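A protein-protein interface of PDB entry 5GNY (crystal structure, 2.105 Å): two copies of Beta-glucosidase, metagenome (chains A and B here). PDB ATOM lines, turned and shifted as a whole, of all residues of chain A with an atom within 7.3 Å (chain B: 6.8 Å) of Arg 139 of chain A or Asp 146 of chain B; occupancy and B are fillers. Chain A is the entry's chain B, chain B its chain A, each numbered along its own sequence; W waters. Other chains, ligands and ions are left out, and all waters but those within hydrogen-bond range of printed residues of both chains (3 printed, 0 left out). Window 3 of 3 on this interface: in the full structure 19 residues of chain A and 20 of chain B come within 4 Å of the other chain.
The backbone NH (N) of Gly 140 of chain B lies close to the backbone NH (N) of Gly 140 of chain A, 3.4 Å away.
The guanidinium group of Arg 139 of chain A is in salt-bridge range of the side-chain carboxylate of Asp 146 of chain B, at 3.3 Å.
The backbone carbonyl oxygen of Asp 138 of chain A lies close to the backbone carbonyl oxygen of Leu 143 of chain B (3.5 Å).
The backbone carbonyl oxygen (O) of Arg 139 of chain A lies close to the backbone carbonyl oxygen (O) of Arg 139 of chain B (3.0 Å).
OD1 of Asn 144 of chain B is in hydrogen-bond range of NH1 of Arg 139 of chain A, at 3.0 Å.
The guanidinium group (NH1) of Arg 139 of chain B lies within salt-bridge range of the side-chain carboxylate (OD2) of Asp 146 of chain A, at 3.5 Å.
NH1 of Arg 139 of chain B lies within hydrogen-bond range of OD1 of Asn 144 of chain A.
The backbone carbonyl oxygen (O) of Leu 143 of chain A lies close to the backbone carbonyl oxygen (O) of Asp 138 of chain B (3.4 Å).
The backbone NH of Asn 144 of chain B is in hydrogen-bond range of the backbone carbonyl oxygen of Asp 138 of chain A (3.2 Å).
The backbone carbonyl oxygen (O) of Asp 138 of chain B lies within hydrogen-bond range of the backbone NH (N) of Asn 144 of chain A (3.3 Å).
N of Asp 146 of chain A lies within hydrogen-bond range of OD1 of Asn 144 of chain A, at 2.9 Å.
The side-chain amide nitrogen of Asn 204 of chain B lies within hydrogen-bond range of the backbone carbonyl oxygen of Leu 143 of chain B, at 3.4 Å.
N of Asp 146 of chain B is in hydrogen-bond range of OD1 of Asn 144 of chain B (3.0 Å).
The backbone carbonyl oxygen (O) of Arg 139 of chain B is in hydrogen-bond range of the side-chain amide nitrogen (ND2) of Asn 144 of chain B (2.8 Å).
Among the printed residues, merely in contact across the chains: Pro 145 of chain A with Arg 139 of chain B (3.3 Å), Gly 140 of chain A with Asp 138 of chain B (3.4 Å), Asp 138 of chain A with Gly 140 of chain B (3.4 Å), Arg 139 of chain A with Pro 145 of chain B (3.5 Å), Gly 140 of chain A with Arg 139 of chain B (3.6 Å), Arg 139 of chain A with Gly 140 of chain B (3.7 Å) and Asp 138 of chain A with Arg 139 of chain B (3.98 Å).
Arg 139 of chain A touches just these residues of chain B: Arg 139 (3.0 Å), Gly 140 (3.7 Å), Asn 144 (3.0 Å), Pro 145 (3.5 Å) and Asp 146 (3.3 Å).
Asp 146 of chain B touches one residue of chain A.
Printed residues of chain B within 4 Å of Asn 144 of chain A: Asp 138 (3.3 Å) and Arg 139 (3.0 Å).
Of the printed residues of chain A, Arg 139 of chain B touches Asp 138 (3.98 Å), Arg 139 (3.0 Å), Gly 140 (3.6 Å), Asn 144 (3.0 Å), Pro 145 (3.3 Å) and Asp 146 (3.5 Å).
Printed residues of chain A within 4 Å of Asn 144 of chain B: Asp 138 (3.2 Å) and Arg 139 (3.0 Å).
Phe 151 of chain B touches none of the printed residues of chain A.
Arg 98 of chain B touches none of the printed residues of chain A.
The nearest residue of chain A that does not touch Asp 146 of chain B is Arg 98 of chain A (7.1 Å).
Of the 17 printed residues of chain A, 7 touch a printed residue of chain B.
Along chain B the printed residues that touch a printed residue of chain A span positions 138 to 146.
Among the printed residues, 17 pairs touch across the chains.
Among the printed residues, Asp or Glu carboxylates within 4 Å of a Lys or Arg side-chain nitrogen of the other chain: Arg 139 of chain A with Asp 146 of chain B and Asp 146 of chain A with Arg 139 of chain B.
Asp 138 of chain A touches Leu 143 of chain B, and with the chains exchanged Leu 143 of chain A touches Asp 138 of chain B.
Asp 138 of chain A touches Asn 144 of chain B, and with the chains exchanged Asn 144 of chain A touches Asp 138 of chain B.
Arg 139 of chain A touches Gly 140 of chain B, and with the chains exchanged Gly 140 of chain A touches Arg 139 of chain B.
Positions printed for both chains: 98, 136, 137, 138, 139, 140, 141, 143, 144, 145, 146 and 150.
Water W2 lies within hydrogen-bond range of OD1 of Asp 146 of chain B (2.7 Å) and NH1 of Arg 139 of chain A (3.0 Å).
Water W1 lies within hydrogen-bond range of the side-chain carboxylate of Asp 146 of chain B, the side-chain amide nitrogen of Asn 144 of chain B and the guanidinium group of Arg 139 of chain A.
Water W3 bridges O of Leu 143 of chain B (3.0 Å) and OD2 of Asp 138 of chain A (3.3 Å).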
ATOM      1  N   GLN A  96      -3.898 -24.060   1.004  1.00  0.00           N
ATOM      2  CA  GLN A  96      -4.025 -23.006   0.005  1.00  0.00           C
ATOM      3  C   GLN A  96      -4.282 -21.646   0.644  1.00  0.00           C
ATOM      4  O   GLN A  96      -4.581 -20.676  -0.049  1.00  0.00           O
ATOM      5  CB  GLN A  96      -5.141 -23.333  -0.990  1.00  0.00           C
ATOM      6  CG  GLN A  96      -4.856 -24.538  -1.867  1.00  0.00           C
ATOM      7  CD  GLN A  96      -3.550 -24.404  -2.630  1.00  0.00           C
ATOM      8  OE1 GLN A  96      -2.604 -25.160  -2.403  1.00  0.00           O
ATOM      9  NE2 GLN A  96      -3.494 -23.440  -3.543  1.00  0.00           N
ATOM     10  N   ARG A  98      -6.690 -20.432   1.956  1.00  0.00           N
ATOM     11  CA  ARG A  98      -8.141 -20.355   2.084  1.00  0.00           C
ATOM     12  C   ARG A  98      -8.769 -21.700   1.749  1.00  0.00           C
ATOM     13  O   ARG A  98      -8.141 -22.547   1.115  1.00  0.00           O
ATOM     14  CB  ARG A  98      -8.721 -19.280   1.163  1.00  0.00           C
ATOM     15  CG  ARG A  98      -8.242 -17.870   1.432  1.00  0.00           C
ATOM     16  CD  ARG A  98      -8.653 -16.947   0.296  1.00  0.00           C
ATOM     17  NE  ARG A  98      -8.136 -17.395  -0.996  1.00  0.00           N
ATOM     18  CZ  ARG A  98      -8.369 -16.776  -2.150  1.00  0.00           C
ATOM     19  NH1 ARG A  98      -9.115 -15.680  -2.181  1.00  0.00           N
ATOM     20  NH2 ARG A  98      -7.855 -17.254  -3.276  1.00  0.00           N
ATOM     21  N   PRO A 133       1.318 -18.581   3.547  1.00  0.00           N
ATOM     22  CA  PRO A 133       1.045 -19.545   2.475  1.00  0.00           C
ATOM     23  C   PRO A 133       1.399 -18.976   1.105  1.00  0.00           C
ATOM     24  O   PRO A 133       1.065 -17.827   0.814  1.00  0.00           O
ATOM     25  CB  PRO A 133      -0.462 -19.786   2.597  1.00  0.00           C
ATOM     26  CG  PRO A 133      -0.762 -19.522   4.027  1.00  0.00           C
ATOM     27  CD  PRO A 133       0.154 -18.399   4.433  1.00  0.00           C
ATOM     28  N   ALA A 134       2.079 -19.773   0.284  1.00  0.00           N
ATOM     29  CA  ALA A 134       2.524 -19.328  -1.031  1.00  0.00           C
ATOM     30  C   ALA A 134       1.340 -19.000  -1.938  1.00  0.00           C
ATOM     31  O   ALA A 134       1.430 -18.123  -2.800  1.00  0.00           O
ATOM     32  CB  ALA A 134       3.407 -20.385  -1.674  1.00  0.00           C
ATOM     33  N   ALA A 135       0.235 -19.708  -1.735  1.00  0.00           N
ATOM     34  CA  ALA A 135      -0.976 -19.479  -2.512  1.00  0.00           C
ATOM     35  C   ALA A 135      -1.512 -18.072  -2.275  1.00  0.00           C
ATOM     36  O   ALA A 135      -2.072 -17.450  -3.178  1.00  0.00           O
ATOM     37  CB  ALA A 135      -2.033 -20.518  -2.167  1.00  0.00           C
ATOM     38  N   LEU A 136      -1.332 -17.569  -1.057  1.00  0.00           N
ATOM     39  CA  LEU A 136      -1.794 -16.229  -0.723  1.00  0.00           C
ATOM     40  C   LEU A 136      -0.797 -15.169  -1.175  1.00  0.00           C
ATOM     41  O   LEU A 136      -1.185 -14.059  -1.533  1.00  0.00           O
ATOM     42  CB  LEU A 136      -2.053 -16.108   0.777  1.00  0.00           C
ATOM     43  CG  LEU A 136      -3.158 -17.019   1.311  1.00  0.00           C
ATOM     44  CD1 LEU A 136      -3.377 -16.762   2.789  1.00  0.00           C
ATOM     45  CD2 LEU A 136      -4.446 -16.813   0.523  1.00  0.00           C
ATOM     46  N   ASP A 137       0.488 -15.511  -1.157  1.00  0.00           N
ATOM     47  CA  ASP A 137       1.512 -14.612  -1.674  1.00  0.00           C
ATOM     48  C   ASP A 137       1.294 -14.377  -3.164  1.00  0.00           C
ATOM     49  O   ASP A 137       1.521 -13.278  -3.668  1.00  0.00           O
ATOM     50  CB  ASP A 137       2.910 -15.177  -1.433  1.00  0.00           C
ATOM     51  CG  ASP A 137       3.997 -14.124  -1.565  1.00  0.00           C
ATOM     52  OD1 ASP A 137       3.784 -12.980  -1.110  1.00  0.00           O
ATOM     53  OD2 ASP A 137       5.066 -14.442  -2.126  1.00  0.00           O
ATOM     54  N   ASP A 138       0.844 -15.417  -3.861  1.00  0.00           N
ATOM     55  CA  ASP A 138       0.582 -15.323  -5.292  1.00  0.00           C
ATOM     56  C   ASP A 138      -0.634 -14.451  -5.585  1.00  0.00           C
ATOM     57  O   ASP A 138      -0.850 -14.041  -6.725  1.00  0.00           O
ATOM     58  CB  ASP A 138       0.388 -16.716  -5.893  1.00  0.00           C
ATOM     59  CG  ASP A 138       1.679 -17.508  -5.945  1.00  0.00           C
ATOM     60  OD1 ASP A 138       2.746 -16.910  -5.698  1.00  0.00           O
ATOM     61  OD2 ASP A 138       1.628 -18.722  -6.236  1.00  0.00           O
ATOM     62  N   ARG A 139      -1.421 -14.170  -4.550  1.00  0.00           N
ATOM     63  CA  ARG A 139      -2.554 -13.262  -4.673  1.00  0.00           C
ATOM     64  C   ARG A 139      -2.214 -11.896  -4.087  1.00  0.00           C
ATOM     65  O   ARG A 139      -3.102 -11.088  -3.820  1.00  0.00           O
ATOM     66  CB  ARG A 139      -3.792 -13.837  -3.980  1.00  0.00           C
ATOM     67  CG  ARG A 139      -4.195 -15.221  -4.451  1.00  0.00           C
ATOM     68  CD  ARG A 139      -4.753 -15.193  -5.866  1.00  0.00           C
ATOM     69  NE  ARG A 139      -5.223 -16.512  -6.290  1.00  0.00           N
ATOM     70  CZ  ARG A 139      -6.303 -16.716  -7.039  1.00  0.00           C
ATOM     71  NH1 ARG A 139      -7.032 -15.687  -7.451  1.00  0.00           N
ATOM     72  NH2 ARG A 139      -6.653 -17.950  -7.378  1.00  0.00           N
ATOM     73  N   GLY A 140      -0.926 -11.646  -3.877  1.00  0.00           N
ATOM     74  CA  GLY A 140      -0.474 -10.351  -3.406  1.00  0.00           C
ATOM     75  C   GLY A 140       0.094 -10.356  -2.001  1.00  0.00           C
ATOM     76  O   GLY A 140       0.788  -9.419  -1.604  1.00  0.00           O
ATOM     77  N   GLY A 141      -0.201 -11.409  -1.248  1.00  0.00           N
ATOM     78  CA  GLY A 141       0.277 -11.523   0.118  1.00  0.00           C
ATOM     79  C   GLY A 141      -0.213 -10.386   0.994  1.00  0.00           C
ATOM     80  O   GLY A 141      -1.402 -10.061   0.992  1.00  0.00           O
ATOM     81  N   TRP A 142       0.709  -9.767   1.728  1.00  0.00           N
ATOM     82  CA  TRP A 142       0.367  -8.668   2.628  1.00  0.00           C
ATOM     83  C   TRP A 142       0.125  -7.354   1.889  1.00  0.00           C
ATOM     84  O   TRP A 142      -0.086  -6.315   2.513  1.00  0.00           O
ATOM     85  CB  TRP A 142       1.468  -8.474   3.676  1.00  0.00           C
ATOM     86  CG  TRP A 142       1.535  -9.595   4.659  1.00  0.00           C
ATOM     87  CD1 TRP A 142       2.474 -10.582   4.716  1.00  0.00           C
ATOM     88  CD2 TRP A 142       0.608  -9.859   5.720  1.00  0.00           C
ATOM     89  NE1 TRP A 142       2.196 -11.439   5.752  1.00  0.00           N
ATOM     90  CE2 TRP A 142       1.055 -11.017   6.384  1.00  0.00           C
ATOM     91  CE3 TRP A 142      -0.552  -9.224   6.175  1.00  0.00           C
ATOM     92  CZ2 TRP A 142       0.381 -11.556   7.478  1.00  0.00           C
ATOM     93  CZ3 TRP A 142      -1.218  -9.760   7.260  1.00  0.00           C
ATOM     94  CH2 TRP A 142      -0.751 -10.914   7.899  1.00  0.00           C
ATOM     95  N   LEU A 143       0.156  -7.400   0.562  1.00  0.00           N
ATOM     96  CA  LEU A 143      -0.116  -6.212  -0.238  1.00  0.00           C
ATOM     97  C   LEU A 143      -1.586  -6.174  -0.655  1.00  0.00           C
ATOM     98  O   LEU A 143      -2.091  -5.144  -1.098  1.00  0.00           O
ATOM     99  CB  LEU A 143       0.796  -6.171  -1.466  1.00  0.00           C
ATOM    100  CG  LEU A 143       2.297  -6.225  -1.175  1.00  0.00           C
ATOM    101  CD1 LEU A 143       3.103  -6.206  -2.466  1.00  0.00           C
ATOM    102  CD2 LEU A 143       2.703  -5.070  -0.271  1.00  0.00           C
ATOM    103  N   ASN A 144      -2.260  -7.309  -0.506  1.00  0.00           N
ATOM    104  CA  ASN A 144      -3.678  -7.428  -0.824  1.00  0.00           C
ATOM    105  C   ASN A 144      -4.527  -7.178   0.419  1.00  0.00           C
ATOM    106  O   ASN A 144      -4.425  -7.914   1.396  1.00  0.00           O
ATOM    107  CB  ASN A 144      -3.973  -8.814  -1.408  1.00  0.00           C
ATOM    108  CG  ASN A 144      -5.375  -8.930  -1.993  1.00  0.00           C
ATOM    109  OD1 ASN A 144      -6.313  -8.271  -1.543  1.00  0.00           O
ATOM    110  ND2 ASN A 144      -5.522  -9.783  -3.000  1.00  0.00           N
ATOM    111  N   PRO A 145      -5.378  -6.141   0.383  1.00  0.00           N
ATOM    112  CA  PRO A 145      -6.207  -5.793   1.542  1.00  0.00           C
ATOM    113  C   PRO A 145      -7.139  -6.925   1.980  1.00  0.00           C
ATOM    114  O   PRO A 145      -7.560  -6.944   3.136  1.00  0.00           O
ATOM    115  CB  PRO A 145      -7.006  -4.581   1.052  1.00  0.00           C
ATOM    116  CG  PRO A 145      -6.956  -4.657  -0.440  1.00  0.00           C
ATOM    117  CD  PRO A 145      -5.619  -5.244  -0.759  1.00  0.00           C
ATOM    118  N   ASP A 146      -7.435  -7.861   1.082  1.00  0.00           N
ATOM    119  CA  ASP A 146      -8.279  -9.005   1.421  1.00  0.00           C
ATOM    120  C   ASP A 146      -7.656  -9.904   2.487  1.00  0.00           C
ATOM    121  O   ASP A 146      -8.353 -10.713   3.098  1.00  0.00           O
ATOM    122  CB  ASP A 146      -8.586  -9.849   0.177  1.00  0.00           C
ATOM    123  CG  ASP A 146      -9.526  -9.156  -0.789  1.00  0.00           C
ATOM    124  OD1 ASP A 146     -10.025  -8.061  -0.461  1.00  0.00           O
ATOM    125  OD2 ASP A 146      -9.776  -9.718  -1.875  1.00  0.00           O
ATOM    126  N   TRP A 150      -8.761 -13.139   4.984  1.00  0.00           N
ATOM    127  CA  TRP A 150      -8.092 -14.436   4.909  1.00  0.00           C
ATOM    128  C   TRP A 150      -7.530 -14.836   6.265  1.00  0.00           C
ATOM    129  O   TRP A 150      -7.610 -15.998   6.671  1.00  0.00           O
ATOM    130  CB  TRP A 150      -6.955 -14.415   3.884  1.00  0.00           C
ATOM    131  CG  TRP A 150      -7.349 -13.999   2.504  1.00  0.00           C
ATOM    132  CD1 TRP A 150      -8.600 -14.022   1.960  1.00  0.00           C
ATOM    133  CD2 TRP A 150      -6.475 -13.503   1.483  1.00  0.00           C
ATOM    134  NE1 TRP A 150      -8.559 -13.568   0.664  1.00  0.00           N
ATOM    135  CE2 TRP A 150      -7.267 -13.240   0.348  1.00  0.00           C
ATOM    136  CE3 TRP A 150      -5.100 -13.254   1.419  1.00  0.00           C
ATOM    137  CZ2 TRP A 150      -6.730 -12.741  -0.837  1.00  0.00           C
ATOM    138  CZ3 TRP A 150      -4.569 -12.756   0.245  1.00  0.00           C
ATOM    139  CH2 TRP A 150      -5.383 -12.507  -0.868  1.00  0.00           C
ATOM    140  N   ARG B  98      -8.111  -2.459 -12.964  1.00  0.00           N
ATOM    141  CA  ARG B  98      -9.493  -2.872 -13.175  1.00  0.00           C
ATOM    142  C   ARG B  98     -10.402  -1.704 -12.834  1.00  0.00           C
ATOM    143  O   ARG B  98      -9.995  -0.781 -12.130  1.00  0.00           O
ATOM    144  CB  ARG B  98      -9.855  -4.081 -12.308  1.00  0.00           C
ATOM    145  CG  ARG B  98      -9.004  -5.313 -12.540  1.00  0.00           C
ATOM    146  CD  ARG B  98      -9.148  -6.284 -11.378  1.00  0.00           C
ATOM    147  NE  ARG B  98     -10.482  -6.881 -11.308  1.00  0.00           N
ATOM    148  CZ  ARG B  98     -10.948  -7.541 -10.251  1.00  0.00           C
ATOM    149  NH1 ARG B  98     -10.194  -7.680  -9.167  1.00  0.00           N
ATOM    150  NH2 ARG B  98     -12.171  -8.053 -10.273  1.00  0.00           N
ATOM    151  N   LEU B 136      -2.514  -3.893  -9.450  1.00  0.00           N
ATOM    152  CA  LEU B 136      -2.653  -5.309  -9.779  1.00  0.00           C
ATOM    153  C   LEU B 136      -1.466  -6.118  -9.264  1.00  0.00           C
ATOM    154  O   LEU B 136      -1.598  -7.301  -8.939  1.00  0.00           O
ATOM    155  CB  LEU B 136      -2.806  -5.496 -11.287  1.00  0.00           C
ATOM    156  CG  LEU B 136      -4.048  -4.849 -11.901  1.00  0.00           C
ATOM    157  CD1 LEU B 136      -4.098  -5.117 -13.397  1.00  0.00           C
ATOM    158  CD2 LEU B 136      -5.315  -5.357 -11.216  1.00  0.00           C
ATOM    159  N   ASP B 137      -0.305  -5.477  -9.194  1.00  0.00           N
ATOM    160  CA  ASP B 137       0.863  -6.100  -8.585  1.00  0.00           C
ATOM    161  C   ASP B 137       0.573  -6.360  -7.110  1.00  0.00           C
ATOM    162  O   ASP B 137       0.994  -7.371  -6.549  1.00  0.00           O
ATOM    163  CB  ASP B 137       2.099  -5.216  -8.744  1.00  0.00           C
ATOM    164  CG  ASP B 137       3.395  -5.982  -8.548  1.00  0.00           C
ATOM    165  OD1 ASP B 137       3.457  -7.167  -8.938  1.00  0.00           O
ATOM    166  OD2 ASP B 137       4.361  -5.393  -8.016  1.00  0.00           O
ATOM    167  N   ASP B 138      -0.174  -5.448  -6.494  1.00  0.00           N
ATOM    168  CA  ASP B 138      -0.551  -5.586  -5.093  1.00  0.00           C
ATOM    169  C   ASP B 138      -1.515  -6.749  -4.880  1.00  0.00           C
ATOM    170  O   ASP B 138      -1.694  -7.213  -3.755  1.00  0.00           O
ATOM    171  CB  ASP B 138      -1.166  -4.284  -4.574  1.00  0.00           C
ATOM    172  CG  ASP B 138      -0.142  -3.168  -4.448  1.00  0.00           C
ATOM    173  OD1 ASP B 138       1.065  -3.456  -4.581  1.00  0.00           O
ATOM    174  OD2 ASP B 138      -0.542  -2.007  -4.214  1.00  0.00           O
ATOM    175  N   ARG B 139      -2.130  -7.220  -5.963  1.00  0.00           N
ATOM    176  CA  ARG B 139      -2.993  -8.392  -5.907  1.00  0.00           C
ATOM    177  C   ARG B 139      -2.275  -9.620  -6.469  1.00  0.00           C
ATOM    178  O   ARG B 139      -2.904 -10.631  -6.788  1.00  0.00           O
ATOM    179  CB  ARG B 139      -4.294  -8.141  -6.674  1.00  0.00           C
ATOM    180  CG  ARG B 139      -5.042  -6.881  -6.251  1.00  0.00           C
ATOM    181  CD  ARG B 139      -5.672  -7.032  -4.878  1.00  0.00           C
ATOM    182  NE  ARG B 139      -6.428  -5.841  -4.491  1.00  0.00           N
ATOM    183  CZ  ARG B 139      -7.593  -5.867  -3.846  1.00  0.00           C
ATOM    184  NH1 ARG B 139      -8.148  -7.026  -3.511  1.00  0.00           N
ATOM    185  NH2 ARG B 139      -8.203  -4.730  -3.537  1.00  0.00           N
ATOM    186  N   GLY B 140      -0.956  -9.529  -6.597  1.00  0.00           N
ATOM    187  CA  GLY B 140      -0.160 -10.673  -7.002  1.00  0.00           C
ATOM    188  C   GLY B 140       0.489 -10.539  -8.365  1.00  0.00           C
ATOM    189  O   GLY B 140       1.427 -11.269  -8.685  1.00  0.00           O
ATOM    190  N   GLY B 141      -0.010  -9.606  -9.167  1.00  0.00           N
ATOM    191  CA  GLY B 141       0.512  -9.394 -10.503  1.00  0.00           C
ATOM    192  C   GLY B 141       0.403 -10.636 -11.363  1.00  0.00           C
ATOM    193  O   GLY B 141      -0.635 -11.292 -11.399  1.00  0.00           O
ATOM    194  N   LEU B 143       1.499 -13.421 -10.876  1.00  0.00           N
ATOM    195  CA  LEU B 143       1.387 -14.635 -10.073  1.00  0.00           C
ATOM    196  C   LEU B 143      -0.077 -14.994  -9.799  1.00  0.00           C
ATOM    197  O   LEU B 143      -0.394 -16.131  -9.444  1.00  0.00           O
ATOM    198  CB  LEU B 143       2.137 -14.478  -8.750  1.00  0.00           C
ATOM    199  CG  LEU B 143       3.621 -14.117  -8.841  1.00  0.00           C
ATOM    200  CD1 LEU B 143       4.234 -14.066  -7.454  1.00  0.00           C
ATOM    201  CD2 LEU B 143       4.356 -15.105  -9.732  1.00  0.00           C
ATOM    202  N   ASN B 144      -0.959 -14.012  -9.951  1.00  0.00           N
ATOM    203  CA  ASN B 144      -2.389 -14.215  -9.747  1.00  0.00           C
ATOM    204  C   ASN B 144      -3.038 -14.717 -11.031  1.00  0.00           C
ATOM    205  O   ASN B 144      -3.063 -14.000 -12.026  1.00  0.00           O
ATOM    206  CB  ASN B 144      -3.048 -12.907  -9.291  1.00  0.00           C
ATOM    207  CG  ASN B 144      -4.465 -13.105  -8.767  1.00  0.00           C
ATOM    208  OD1 ASN B 144      -5.179 -14.027  -9.171  1.00  0.00           O
ATOM    209  ND2 ASN B 144      -4.881 -12.227  -7.865  1.00  0.00           N
ATOM    210  N   PRO B 145      -3.571 -15.947 -11.017  1.00  0.00           N
ATOM    211  CA  PRO B 145      -4.177 -16.500 -12.236  1.00  0.00           C
ATOM    212  C   PRO B 145      -5.327 -15.642 -12.781  1.00  0.00           C
ATOM    213  O   PRO B 145      -5.612 -15.700 -13.977  1.00  0.00           O
ATOM    214  CB  PRO B 145      -4.679 -17.882 -11.787  1.00  0.00           C
ATOM    215  CG  PRO B 145      -4.781 -17.798 -10.295  1.00  0.00           C
ATOM    216  CD  PRO B 145      -3.684 -16.867  -9.871  1.00  0.00           C
ATOM    217  N   ASP B 146      -5.951 -14.837 -11.927  1.00  0.00           N
ATOM    218  CA  ASP B 146      -7.024 -13.948 -12.368  1.00  0.00           C
ATOM    219  C   ASP B 146      -6.558 -12.891 -13.370  1.00  0.00           C
ATOM    220  O   ASP B 146      -7.385 -12.282 -14.051  1.00  0.00           O
ATOM    221  CB  ASP B 146      -7.678 -13.248 -11.172  1.00  0.00           C
ATOM    222  CG  ASP B 146      -8.497 -14.193 -10.311  1.00  0.00           C
ATOM    223  OD1 ASP B 146      -8.610 -15.383 -10.668  1.00  0.00           O
ATOM    224  OD2 ASP B 146      -9.044 -13.737  -9.286  1.00  0.00           O
ATOM    225  N   ILE B 147      -5.248 -12.670 -13.464  1.00  0.00           N
ATOM    226  CA  ILE B 147      -4.727 -11.621 -14.341  1.00  0.00           C
ATOM    227  C   ILE B 147      -5.066 -11.898 -15.808  1.00  0.00           C
ATOM    228  O   ILE B 147      -5.137 -10.973 -16.615  1.00  0.00           O
ATOM    229  CB  ILE B 147      -3.195 -11.446 -14.193  1.00  0.00           C
ATOM    230  CG1 ILE B 147      -2.735 -10.158 -14.884  1.00  0.00           C
ATOM    231  CG2 ILE B 147      -2.449 -12.647 -14.754  1.00  0.00           C
ATOM    232  CD1 ILE B 147      -1.366  -9.693 -14.467  1.00  0.00           C
ATOM    233  N   ALA B 148      -5.292 -13.165 -16.144  1.00  0.00           N
ATOM    234  CA  ALA B 148      -5.718 -13.530 -17.490  1.00  0.00           C
ATOM    235  C   ALA B 148      -7.028 -12.827 -17.826  1.00  0.00           C
ATOM    236  O   ALA B 148      -7.199 -12.303 -18.927  1.00  0.00           O
ATOM    237  CB  ALA B 148      -5.870 -15.043 -17.617  1.00  0.00           C
ATOM    238  N   ASP B 149      -7.942 -12.806 -16.859  1.00  0.00           N
ATOM    239  CA  ASP B 149      -9.224 -12.128 -17.018  1.00  0.00           C
ATOM    240  C   ASP B 149      -9.061 -10.610 -17.016  1.00  0.00           C
ATOM    241  O   ASP B 149      -9.662  -9.916 -17.842  1.00  0.00           O
ATOM    242  CB  ASP B 149     -10.192 -12.550 -15.910  1.00  0.00           C
ATOM    243  CG  ASP B 149     -10.516 -14.028 -15.953  1.00  0.00           C
ATOM    244  OD1 ASP B 149     -10.671 -14.575 -17.066  1.00  0.00           O
ATOM    245  OD2 ASP B 149     -10.609 -14.645 -14.870  1.00  0.00           O
ATOM    246  N   TRP B 150      -8.260 -10.097 -16.082  1.00  0.00           N
ATOM    247  CA  TRP B 150      -8.008  -8.658 -16.007  1.00  0.00           C
ATOM    248  C   TRP B 150      -7.413  -8.141 -17.310  1.00  0.00           C
ATOM    249  O   TRP B 150      -7.702  -7.022 -17.739  1.00  0.00           O
ATOM    250  CB  TRP B 150      -7.051  -8.312 -14.863  1.00  0.00           C
ATOM    251  CG  TRP B 150      -7.440  -8.822 -13.516  1.00  0.00           C
ATOM    252  CD1 TRP B 150      -8.689  -9.182 -13.093  1.00  0.00           C
ATOM    253  CD2 TRP B 150      -6.562  -9.032 -12.403  1.00  0.00           C
ATOM    254  NE1 TRP B 150      -8.640  -9.602 -11.783  1.00  0.00           N
ATOM    255  CE2 TRP B 150      -7.347  -9.519 -11.338  1.00  0.00           C
ATOM    256  CE3 TRP B 150      -5.188  -8.853 -12.204  1.00  0.00           C
ATOM    257  CZ2 TRP B 150      -6.801  -9.831 -10.095  1.00  0.00           C
ATOM    258  CZ3 TRP B 150      -4.649  -9.165 -10.971  1.00  0.00           C
ATOM    259  CH2 TRP B 150      -5.454  -9.648  -9.931  1.00  0.00           C
ATOM    260  N   PHE B 151      -6.559  -8.956 -17.921  1.00  0.00           N
ATOM    261  CA  PHE B 151      -5.854  -8.553 -19.131  1.00  0.00           C
ATOM    262  C   PHE B 151      -6.766  -8.586 -20.354  1.00  0.00           C
ATOM    263  O   PHE B 151      -6.653  -7.746 -21.244  1.00  0.00           O
ATOM    264  CB  PHE B 151      -4.638  -9.449 -19.362  1.00  0.00           C
ATOM    265  CG  PHE B 151      -3.810  -9.050 -20.547  1.00  0.00           C
ATOM    266  CD1 PHE B 151      -3.173  -7.821 -20.581  1.00  0.00           C
ATOM    267  CD2 PHE B 151      -3.674  -9.902 -21.628  1.00  0.00           C
ATOM    268  CE1 PHE B 151      -2.408  -7.448 -21.672  1.00  0.00           C
ATOM    269  CE2 PHE B 151      -2.911  -9.537 -22.724  1.00  0.00           C
ATOM    270  CZ  PHE B 151      -2.276  -8.308 -22.743  1.00  0.00           C
ATOM    271  N   ASN B 204       1.110 -17.730 -16.408  1.00  0.00           N
ATOM    272  CA  ASN B 204       0.015 -16.762 -16.418  1.00  0.00           C
ATOM    273  C   ASN B 204       0.140 -15.712 -17.520  1.00  0.00           C
ATOM    274  O   ASN B 204      -0.869 -15.209 -18.013  1.00  0.00           O
ATOM    275  CB  ASN B 204      -0.098 -16.072 -15.060  1.00  0.00           C
ATOM    276  CG  ASN B 204      -0.758 -16.950 -14.018  1.00  0.00           C
ATOM    277  OD1 ASN B 204      -1.610 -17.780 -14.342  1.00  0.00           O
ATOM    278  ND2 ASN B 204      -0.376 -16.771 -12.758  1.00  0.00           N
ATOM    279  N   ARG B 207      -1.306 -17.604 -20.383  1.00  0.00           N
ATOM    280  CA  ARG B 207      -2.758 -17.659 -20.217  1.00  0.00           C
ATOM    281  C   ARG B 207      -3.409 -16.324 -20.552  1.00  0.00           C
ATOM    282  O   ARG B 207      -4.458 -16.277 -21.193  1.00  0.00           O
ATOM    283  CB  ARG B 207      -3.131 -18.068 -18.792  1.00  0.00           C
ATOM    284  CG  ARG B 207      -2.820 -19.508 -18.442  1.00  0.00           C
ATOM    285  CD  ARG B 207      -3.278 -19.836 -17.023  1.00  0.00           C
ATOM    286  NE  ARG B 207      -4.710 -19.608 -16.835  1.00  0.00           N
ATOM    287  CZ  ARG B 207      -5.230 -18.598 -16.143  1.00  0.00           C
ATOM    288  NH1 ARG B 207      -4.441 -17.707 -15.554  1.00  0.00           N
ATOM    289  NH2 ARG B 207      -6.545 -18.483 -16.034  1.00  0.00           N
HETATM  290  O   HOH W   1      -7.910 -12.430  -6.975  1.00  0.00           O
HETATM  291  O   HOH W   2      -9.456 -16.960  -8.653  1.00  0.00           O
HETATM  292  O   HOH W   3      -0.716 -19.007  -8.611  1.00  0.00           O
